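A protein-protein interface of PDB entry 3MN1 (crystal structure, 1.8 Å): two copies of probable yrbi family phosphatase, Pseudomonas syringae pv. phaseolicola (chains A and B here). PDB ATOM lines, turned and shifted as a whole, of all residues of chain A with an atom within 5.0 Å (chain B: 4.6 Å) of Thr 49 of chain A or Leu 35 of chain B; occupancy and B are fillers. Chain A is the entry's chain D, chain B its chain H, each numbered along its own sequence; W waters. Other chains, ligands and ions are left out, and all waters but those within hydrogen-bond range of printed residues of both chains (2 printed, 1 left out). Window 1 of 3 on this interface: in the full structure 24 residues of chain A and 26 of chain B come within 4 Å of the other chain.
Printed residues of chain B that touch a printed residue of chain A: Asp 27, Gly 33, Arg 34, Leu 35, Tyr 36, Phe 37, Asp 118 and Asp 119.
Along chain B the printed residues that touch a printed residue of chain A span positions 27 to 119.
Among the printed residues, no Asp or Glu carboxylate lies within 4 Å of a Lys or Arg side-chain nitrogen of the other chain.
The side-chain amide oxygen (OD1) of Asn 48 of chain A lies within hydrogen-bond range of the backbone NH (N) of Asp 51 of chain A (3.0 Å).
The side-chain amide oxygen of Asn 48 of chain A lies within hydrogen-bond range of the backbone NH of Leu 50 of chain A, 2.9 Å away.
The backbone carbonyl oxygen of Asn 48 of chain A lies within hydrogen-bond range of the guanidinium group of Arg 79 of chain A (3.3 Å).
The side-chain carboxylate of Asp 27 of chain B is in salt-bridge range of the side-chain amino group of Lys 45 of chain B (2.7 Å).
1 position is printed for both chains.
The backbone carbonyl oxygen (O) of Gly 33 of chain B sits at hydrogen-bond distance from the backbone NH (N) of Thr 49 of chain A, at 3.0 Å.
The backbone carbonyl oxygen (O) of Leu 35 of chain B lies close to the backbone carbonyl oxygen (O) of Lys 45 of chain A (3.5 Å).
The backbone carbonyl oxygen (O) of Lys 45 of chain A lies within hydrogen-bond range of the backbone NH (N) of Phe 37 of chain B.
O of Phe 47 of chain A sits at hydrogen-bond distance from N of Leu 35 of chain B, at 2.7 Å.
Water W2 bridges the side-chain hydroxyl (OG1) of Thr 46 of chain A (2.7 Å) and the guanidinium group (NE) of Arg 34 of chain B (3.2 Å).
Water W1 lies within hydrogen-bond range of OD2 of Asp 118 of chain B, O of Asp 27 of chain B and OG1 of Thr 49 of chain A.
Among the printed residues, pairs that only touch across the chains: Thr 46 of chain A with Leu 35 of chain B (3.1 Å), Thr 46 of chain A with Tyr 36 of chain B (3.2 Å), Phe 47 of chain A with Arg 34 of chain B (3.2 Å), Leu 50 of chain A with Asp 119 of chain B (3.3 Å), Gln 53 of chain A with Asp 119 of chain B (3.4 Å), Lys 45 of chain A with Tyr 36 of chain B (3.4 Å), Asn 48 of chain A with Gly 33 of chain B (3.4 Å), Thr 49 of chain A with Leu 35 of chain B (3.6 Å), Arg 79 of chain A with Leu 35 of chain B (3.6 Å), Phe 47 of chain A with Gly 33 of chain B (3.7 Å), Phe 47 of chain A with Phe 37 of chain B (3.8 Å), Thr 49 of chain A with Asp 27 of chain B (3.9 Å) and Leu 50 of chain A with Asp 118 of chain B (3.97 Å).
Of the printed residues of chain B, Thr 49 of chain A touches Asp 27 (3.9 Å), Gly 33 (3.0 Å) and Leu 35 (3.6 Å).
Printed residues of chain A within 4 Å of Leu 35 of chain B: Lys 45, Thr 46, Phe 47, Thr 49 and Arg 79.
Of the printed residues of chain B, Gln 53 of chain A touches Asp 119.
Of the printed residues of chain B, Arg 79 of chain A touches Leu 35 (3.6 Å).
Printed residues of chain B within 4 Å of Thr 46 of chain A: Leu 35 and Tyr 36.
Of the printed residues of chain B, Leu 50 of chain A touches Asp 118 (3.97 Å) and Asp 119 (3.3 Å).
Lys 45 of chain B touches none of the printed residues of chain A.
The nearest printed residue of chain A that does not touch Leu 35 of chain B is Asn 48 of chain A (4.7 Å).
The nearest printed residue of chain A that does not touch Phe 37 of chain B is Arg 79 of chain A (4.7 Å).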
ATOM      1  N   LYS A  45      -2.647 -17.209  -8.031  1.00  0.00           N
ATOM      2  CA  LYS A  45      -1.403 -16.618  -7.559  1.00  0.00           C
ATOM      3  C   LYS A  45      -1.550 -15.106  -7.475  1.00  0.00           C
ATOM      4  O   LYS A  45      -2.323 -14.516  -8.234  1.00  0.00           O
ATOM      5  CB  LYS A  45      -0.251 -17.017  -8.479  1.00  0.00           C
ATOM      6  CG  LYS A  45       1.127 -16.936  -7.799  1.00  0.00           C
ATOM      7  CD  LYS A  45       2.179 -17.673  -8.626  1.00  0.00           C
ATOM      8  CE  LYS A  45       1.926 -19.173  -8.626  1.00  0.00           C
ATOM      9  NZ  LYS A  45       2.361 -19.820  -7.342  1.00  0.00           N
ATOM     10  N   THR A  46      -0.812 -14.485  -6.554  1.00  0.00           N
ATOM     11  CA  THR A  46      -0.891 -13.037  -6.367  1.00  0.00           C
ATOM     12  C   THR A  46       0.455 -12.401  -6.622  1.00  0.00           C
ATOM     13  O   THR A  46       1.478 -12.844  -6.089  1.00  0.00           O
ATOM     14  CB  THR A  46      -1.385 -12.659  -4.946  1.00  0.00           C
ATOM     15  OG1 THR A  46      -0.436 -13.091  -3.965  1.00  0.00           O
ATOM     16  CG2 THR A  46      -2.724 -13.315  -4.661  1.00  0.00           C
ATOM     17  N   PHE A  47       0.450 -11.380  -7.467  1.00  0.00           N
ATOM     18  CA  PHE A  47       1.619 -10.558  -7.686  1.00  0.00           C
ATOM     19  C   PHE A  47       1.354  -9.151  -7.164  1.00  0.00           C
ATOM     20  O   PHE A  47       0.274  -8.860  -6.666  1.00  0.00           O
ATOM     21  CB  PHE A  47       1.951 -10.529  -9.178  1.00  0.00           C
ATOM     22  CG  PHE A  47       2.152 -11.896  -9.752  1.00  0.00           C
ATOM     23  CD1 PHE A  47       3.297 -12.614  -9.463  1.00  0.00           C
ATOM     24  CD2 PHE A  47       1.174 -12.476 -10.540  1.00  0.00           C
ATOM     25  CE1 PHE A  47       3.485 -13.891  -9.991  1.00  0.00           C
ATOM     26  CE2 PHE A  47       1.353 -13.741 -11.072  1.00  0.00           C
ATOM     27  CZ  PHE A  47       2.501 -14.457 -10.785  1.00  0.00           C
ATOM     28  N   ASN A  48       2.343  -8.284  -7.289  1.00  0.00           N
ATOM     29  CA  ASN A  48       2.255  -6.964  -6.676  1.00  0.00           C
ATOM     30  C   ASN A  48       2.514  -5.872  -7.711  1.00  0.00           C
ATOM     31  O   ASN A  48       3.447  -5.968  -8.508  1.00  0.00           O
ATOM     32  CB  ASN A  48       3.266  -6.905  -5.535  1.00  0.00           C
ATOM     33  CG  ASN A  48       3.455  -5.506  -4.988  1.00  0.00           C
ATOM     34  OD1 ASN A  48       4.258  -4.726  -5.498  1.00  0.00           O
ATOM     35  ND2 ASN A  48       2.748  -5.198  -3.924  1.00  0.00           N
ATOM     36  N   THR A  49       1.682  -4.836  -7.722  1.00  0.00           N
ATOM     37  CA  THR A  49       1.811  -3.817  -8.756  1.00  0.00           C
ATOM     38  C   THR A  49       3.102  -2.998  -8.665  1.00  0.00           C
ATOM     39  O   THR A  49       3.645  -2.593  -9.688  1.00  0.00           O
ATOM     40  CB  THR A  49       0.576  -2.886  -8.818  1.00  0.00           C
ATOM     41  OG1 THR A  49       0.242  -2.440  -7.499  1.00  0.00           O
ATOM     42  CG2 THR A  49      -0.609  -3.638  -9.412  1.00  0.00           C
ATOM     43  N   LEU A  50       3.598  -2.757  -7.461  1.00  0.00           N
ATOM     44  CA  LEU A  50       4.853  -1.993  -7.348  1.00  0.00           C
ATOM     45  C   LEU A  50       5.969  -2.780  -8.024  1.00  0.00           C
ATOM     46  O   LEU A  50       6.860  -2.216  -8.669  1.00  0.00           O
ATOM     47  CB  LEU A  50       5.226  -1.782  -5.880  1.00  0.00           C
ATOM     48  CG  LEU A  50       4.439  -0.741  -5.076  1.00  0.00           C
ATOM     49  CD1 LEU A  50       4.896  -0.747  -3.611  1.00  0.00           C
ATOM     50  CD2 LEU A  50       4.632   0.618  -5.698  1.00  0.00           C
ATOM     51  N   ASP A  51       5.941  -4.096  -7.856  1.00  0.00           N
ATOM     52  CA  ASP A  51       6.973  -4.947  -8.484  1.00  0.00           C
ATOM     53  C   ASP A  51       6.947  -4.880 -10.007  1.00  0.00           C
ATOM     54  O   ASP A  51       8.012  -4.829 -10.651  1.00  0.00           O
ATOM     55  CB  ASP A  51       6.792  -6.407  -8.048  1.00  0.00           C
ATOM     56  CG  ASP A  51       7.141  -6.650  -6.587  1.00  0.00           C
ATOM     57  OD1 ASP A  51       7.901  -5.871  -5.979  1.00  0.00           O
ATOM     58  OD2 ASP A  51       6.688  -7.690  -6.048  1.00  0.00           O
ATOM     59  N   GLY A  52       5.747  -4.904 -10.594  1.00  0.00           N
ATOM     60  CA  GLY A  52       5.585  -4.795 -12.041  1.00  0.00           C
ATOM     61  C   GLY A  52       6.235  -3.540 -12.599  1.00  0.00           C
ATOM     62  O   GLY A  52       6.999  -3.595 -13.565  1.00  0.00           O
ATOM     63  N   GLN A  53       5.951  -2.409 -11.962  1.00  0.00           N
ATOM     64  CA  GLN A  53       6.529  -1.115 -12.350  1.00  0.00           C
ATOM     65  C   GLN A  53       8.060  -1.144 -12.242  1.00  0.00           C
ATOM     66  O   GLN A  53       8.771  -0.642 -13.116  1.00  0.00           O
ATOM     67  CB  GLN A  53       5.935  -0.007 -11.464  1.00  0.00           C
ATOM     68  CG  GLN A  53       6.548   1.364 -11.645  1.00  0.00           C
ATOM     69  CD  GLN A  53       6.195   1.997 -12.970  1.00  0.00           C
ATOM     70  OE1 GLN A  53       5.158   1.696 -13.568  1.00  0.00           O
ATOM     71  NE2 GLN A  53       7.050   2.898 -13.436  1.00  0.00           N
ATOM     72  N   ARG A  79       2.091 -13.762 -16.558  1.00  0.00           N
ATOM     73  CA  ARG A  79       2.662 -12.635 -15.826  1.00  0.00           C
ATOM     74  C   ARG A  79       4.004 -12.226 -16.451  1.00  0.00           C
ATOM     75  O   ARG A  79       4.259 -11.042 -16.698  1.00  0.00           O
ATOM     76  CB  ARG A  79       2.824 -13.000 -14.338  1.00  0.00           C
ATOM     77  CG  ARG A  79       3.438 -11.893 -13.483  1.00  0.00           C
ATOM     78  CD  ARG A  79       2.586 -10.608 -13.449  1.00  0.00           C
ATOM     79  NE  ARG A  79       3.122  -9.635 -12.477  1.00  0.00           N
ATOM     80  CZ  ARG A  79       2.663  -8.388 -12.306  1.00  0.00           C
ATOM     81  NH1 ARG A  79       1.641  -7.940 -13.025  1.00  0.00           N
ATOM     82  NH2 ARG A  79       3.224  -7.589 -11.403  1.00  0.00           N
ATOM     83  N   ASP B  27      -5.375   0.053  -8.067  1.00  0.00           N
ATOM     84  CA  ASP B  27      -4.492  -0.937  -7.469  1.00  0.00           C
ATOM     85  C   ASP B  27      -3.431  -0.289  -6.566  1.00  0.00           C
ATOM     86  O   ASP B  27      -2.645   0.567  -6.996  1.00  0.00           O
ATOM     87  CB  ASP B  27      -3.873  -1.739  -8.602  1.00  0.00           C
ATOM     88  CG  ASP B  27      -4.923  -2.480  -9.391  1.00  0.00           C
ATOM     89  OD1 ASP B  27      -5.383  -3.527  -8.892  1.00  0.00           O
ATOM     90  OD2 ASP B  27      -5.314  -2.004 -10.481  1.00  0.00           O
ATOM     91  N   GLY B  33      -2.746  -3.683  -3.485  1.00  0.00           N
ATOM     92  CA  GLY B  33      -1.694  -3.761  -4.500  1.00  0.00           C
ATOM     93  C   GLY B  33      -1.464  -5.175  -5.009  1.00  0.00           C
ATOM     94  O   GLY B  33      -0.687  -5.377  -5.932  1.00  0.00           O
ATOM     95  N   ARG B  34      -2.144  -6.152  -4.448  1.00  0.00           N
ATOM     96  CA  ARG B  34      -2.030  -7.505  -4.923  1.00  0.00           C
ATOM     97  C   ARG B  34      -2.905  -7.712  -6.147  1.00  0.00           C
ATOM     98  O   ARG B  34      -4.024  -7.280  -6.154  1.00  0.00           O
ATOM     99  CB  ARG B  34      -2.579  -8.467  -3.884  1.00  0.00           C
ATOM    100  CG  ARG B  34      -1.792  -8.612  -2.636  1.00  0.00           C
ATOM    101  CD  ARG B  34      -2.494  -9.540  -1.690  1.00  0.00           C
ATOM    102  NE  ARG B  34      -1.599 -10.094  -0.713  1.00  0.00           N
ATOM    103  CZ  ARG B  34      -1.270  -9.495   0.422  1.00  0.00           C
ATOM    104  NH1 ARG B  34      -0.400 -10.062   1.252  1.00  0.00           N
ATOM    105  NH2 ARG B  34      -1.798  -8.332   0.735  1.00  0.00           N
ATOM    106  N   LEU B  35      -2.360  -8.378  -7.149  1.00  0.00           N
ATOM    107  CA  LEU B  35      -3.089  -8.808  -8.340  1.00  0.00           C
ATOM    108  C   LEU B  35      -3.259 -10.324  -8.243  1.00  0.00           C
ATOM    109  O   LEU B  35      -2.271 -11.061  -8.274  1.00  0.00           O
ATOM    110  CB  LEU B  35      -2.274  -8.464  -9.599  1.00  0.00           C
ATOM    111  CG  LEU B  35      -1.962  -6.971  -9.779  1.00  0.00           C
ATOM    112  CD1 LEU B  35      -1.055  -6.791 -10.996  1.00  0.00           C
ATOM    113  CD2 LEU B  35      -3.245  -6.197  -9.961  1.00  0.00           C
ATOM    114  N   TYR B  36      -4.502 -10.782  -8.133  1.00  0.00           N
ATOM    115  CA  TYR B  36      -4.807 -12.209  -8.083  1.00  0.00           C
ATOM    116  C   TYR B  36      -5.158 -12.712  -9.487  1.00  0.00           C
ATOM    117  O   TYR B  36      -6.005 -12.123 -10.161  1.00  0.00           O
ATOM    118  CB  TYR B  36      -6.046 -12.446  -7.235  1.00  0.00           C
ATOM    119  CG  TYR B  36      -5.941 -12.106  -5.765  1.00  0.00           C
ATOM    120  CD1 TYR B  36      -5.874 -13.110  -4.815  1.00  0.00           C
ATOM    121  CD2 TYR B  36      -5.968 -10.781  -5.322  1.00  0.00           C
ATOM    122  CE1 TYR B  36      -5.809 -12.820  -3.469  1.00  0.00           C
ATOM    123  CE2 TYR B  36      -5.911 -10.482  -3.968  1.00  0.00           C
ATOM    124  CZ  TYR B  36      -5.830 -11.508  -3.046  1.00  0.00           C
ATOM    125  OH  TYR B  36      -5.767 -11.221  -1.691  1.00  0.00           O
ATOM    126  N   PHE B  37      -4.539 -13.805  -9.915  1.00  0.00           N
ATOM    127  CA  PHE B  37      -4.858 -14.381 -11.219  1.00  0.00           C
ATOM    128  C   PHE B  37      -5.159 -15.867 -11.083  1.00  0.00           C
ATOM    129  O   PHE B  37      -4.474 -16.593 -10.352  1.00  0.00           O
ATOM    130  CB  PHE B  37      -3.698 -14.211 -12.192  1.00  0.00           C
ATOM    131  CG  PHE B  37      -3.386 -12.789 -12.537  1.00  0.00           C
ATOM    132  CD1 PHE B  37      -4.068 -12.151 -13.564  1.00  0.00           C
ATOM    133  CD2 PHE B  37      -2.368 -12.105 -11.873  1.00  0.00           C
ATOM    134  CE1 PHE B  37      -3.761 -10.846 -13.916  1.00  0.00           C
ATOM    135  CE2 PHE B  37      -2.056 -10.797 -12.213  1.00  0.00           C
ATOM    136  CZ  PHE B  37      -2.750 -10.167 -13.242  1.00  0.00           C
ATOM    137  N   LYS B  45     -10.112  -9.256  -7.364  1.00  0.00           N
ATOM    138  CA  LYS B  45      -9.560  -8.052  -6.754  1.00  0.00           C
ATOM    139  C   LYS B  45     -10.196  -7.849  -5.399  1.00  0.00           C
ATOM    140  O   LYS B  45     -11.336  -8.280  -5.180  1.00  0.00           O
ATOM    141  CB  LYS B  45      -9.813  -6.844  -7.648  1.00  0.00           C
ATOM    142  CG  LYS B  45      -8.886  -5.666  -7.351  1.00  0.00           C
ATOM    143  CD  LYS B  45      -8.945  -4.630  -8.467  1.00  0.00           C
ATOM    144  CE  LYS B  45      -8.527  -5.229  -9.799  1.00  0.00           C
ATOM    145  NZ  LYS B  45      -7.027  -5.431  -9.899  1.00  0.00           N
ATOM    146  N   ARG B  71      -4.891   0.288 -15.429  1.00  0.00           N
ATOM    147  CA  ARG B  71      -5.439  -1.041 -15.723  1.00  0.00           C
ATOM    148  C   ARG B  71      -6.937  -0.966 -16.046  1.00  0.00           C
ATOM    149  O   ARG B  71      -7.562   0.094 -15.940  1.00  0.00           O
ATOM    150  CB  ARG B  71      -5.189  -2.056 -14.580  1.00  0.00           C
ATOM    151  CG  ARG B  71      -3.719  -2.263 -14.220  1.00  0.00           C
ATOM    152  CD  ARG B  71      -3.500  -3.282 -13.083  1.00  0.00           C
ATOM    153  NE  ARG B  71      -4.027  -4.614 -13.412  1.00  0.00           N
ATOM    154  CZ  ARG B  71      -3.350  -5.545 -14.076  1.00  0.00           C
ATOM    155  NH1 ARG B  71      -2.110  -5.298 -14.496  1.00  0.00           N
ATOM    156  NH2 ARG B  71      -3.915  -6.721 -14.325  1.00  0.00           N
ATOM    157  N   ASP B 118      -0.372   5.934  -5.510  1.00  0.00           N
ATOM    158  CA  ASP B 118       0.550   4.958  -4.915  1.00  0.00           C
ATOM    159  C   ASP B 118       1.820   4.684  -5.707  1.00  0.00           C
ATOM    160  O   ASP B 118       2.754   4.074  -5.173  1.00  0.00           O
ATOM    161  CB  ASP B 118      -0.154   3.634  -4.644  1.00  0.00           C
ATOM    162  CG  ASP B 118      -0.134   2.713  -5.833  1.00  0.00           C
ATOM    163  OD1 ASP B 118      -0.678   3.100  -6.890  1.00  0.00           O
ATOM    164  OD2 ASP B 118       0.423   1.595  -5.703  1.00  0.00           O
ATOM    165  N   ASP B 119       1.861   5.069  -6.979  1.00  0.00           N
ATOM    166  CA  ASP B 119       3.089   4.816  -7.738  1.00  0.00           C
ATOM    167  C   ASP B 119       3.376   5.911  -8.766  1.00  0.00           C
ATOM    168  O   ASP B 119       2.608   6.866  -8.923  1.00  0.00           O
ATOM    169  CB  ASP B 119       3.040   3.421  -8.386  1.00  0.00           C
ATOM    170  CG  ASP B 119       4.421   2.795  -8.553  1.00  0.00           C
ATOM    171  OD1 ASP B 119       5.445   3.503  -8.388  1.00  0.00           O
ATOM    172  OD2 ASP B 119       4.483   1.569  -8.842  1.00  0.00           O
HETATM  173  O   HOH W   1       0.070   0.495  -8.366  1.00  0.00           O
HETATM  174  O   HOH W   2      -1.402 -13.198  -1.434  1.00  0.00           O
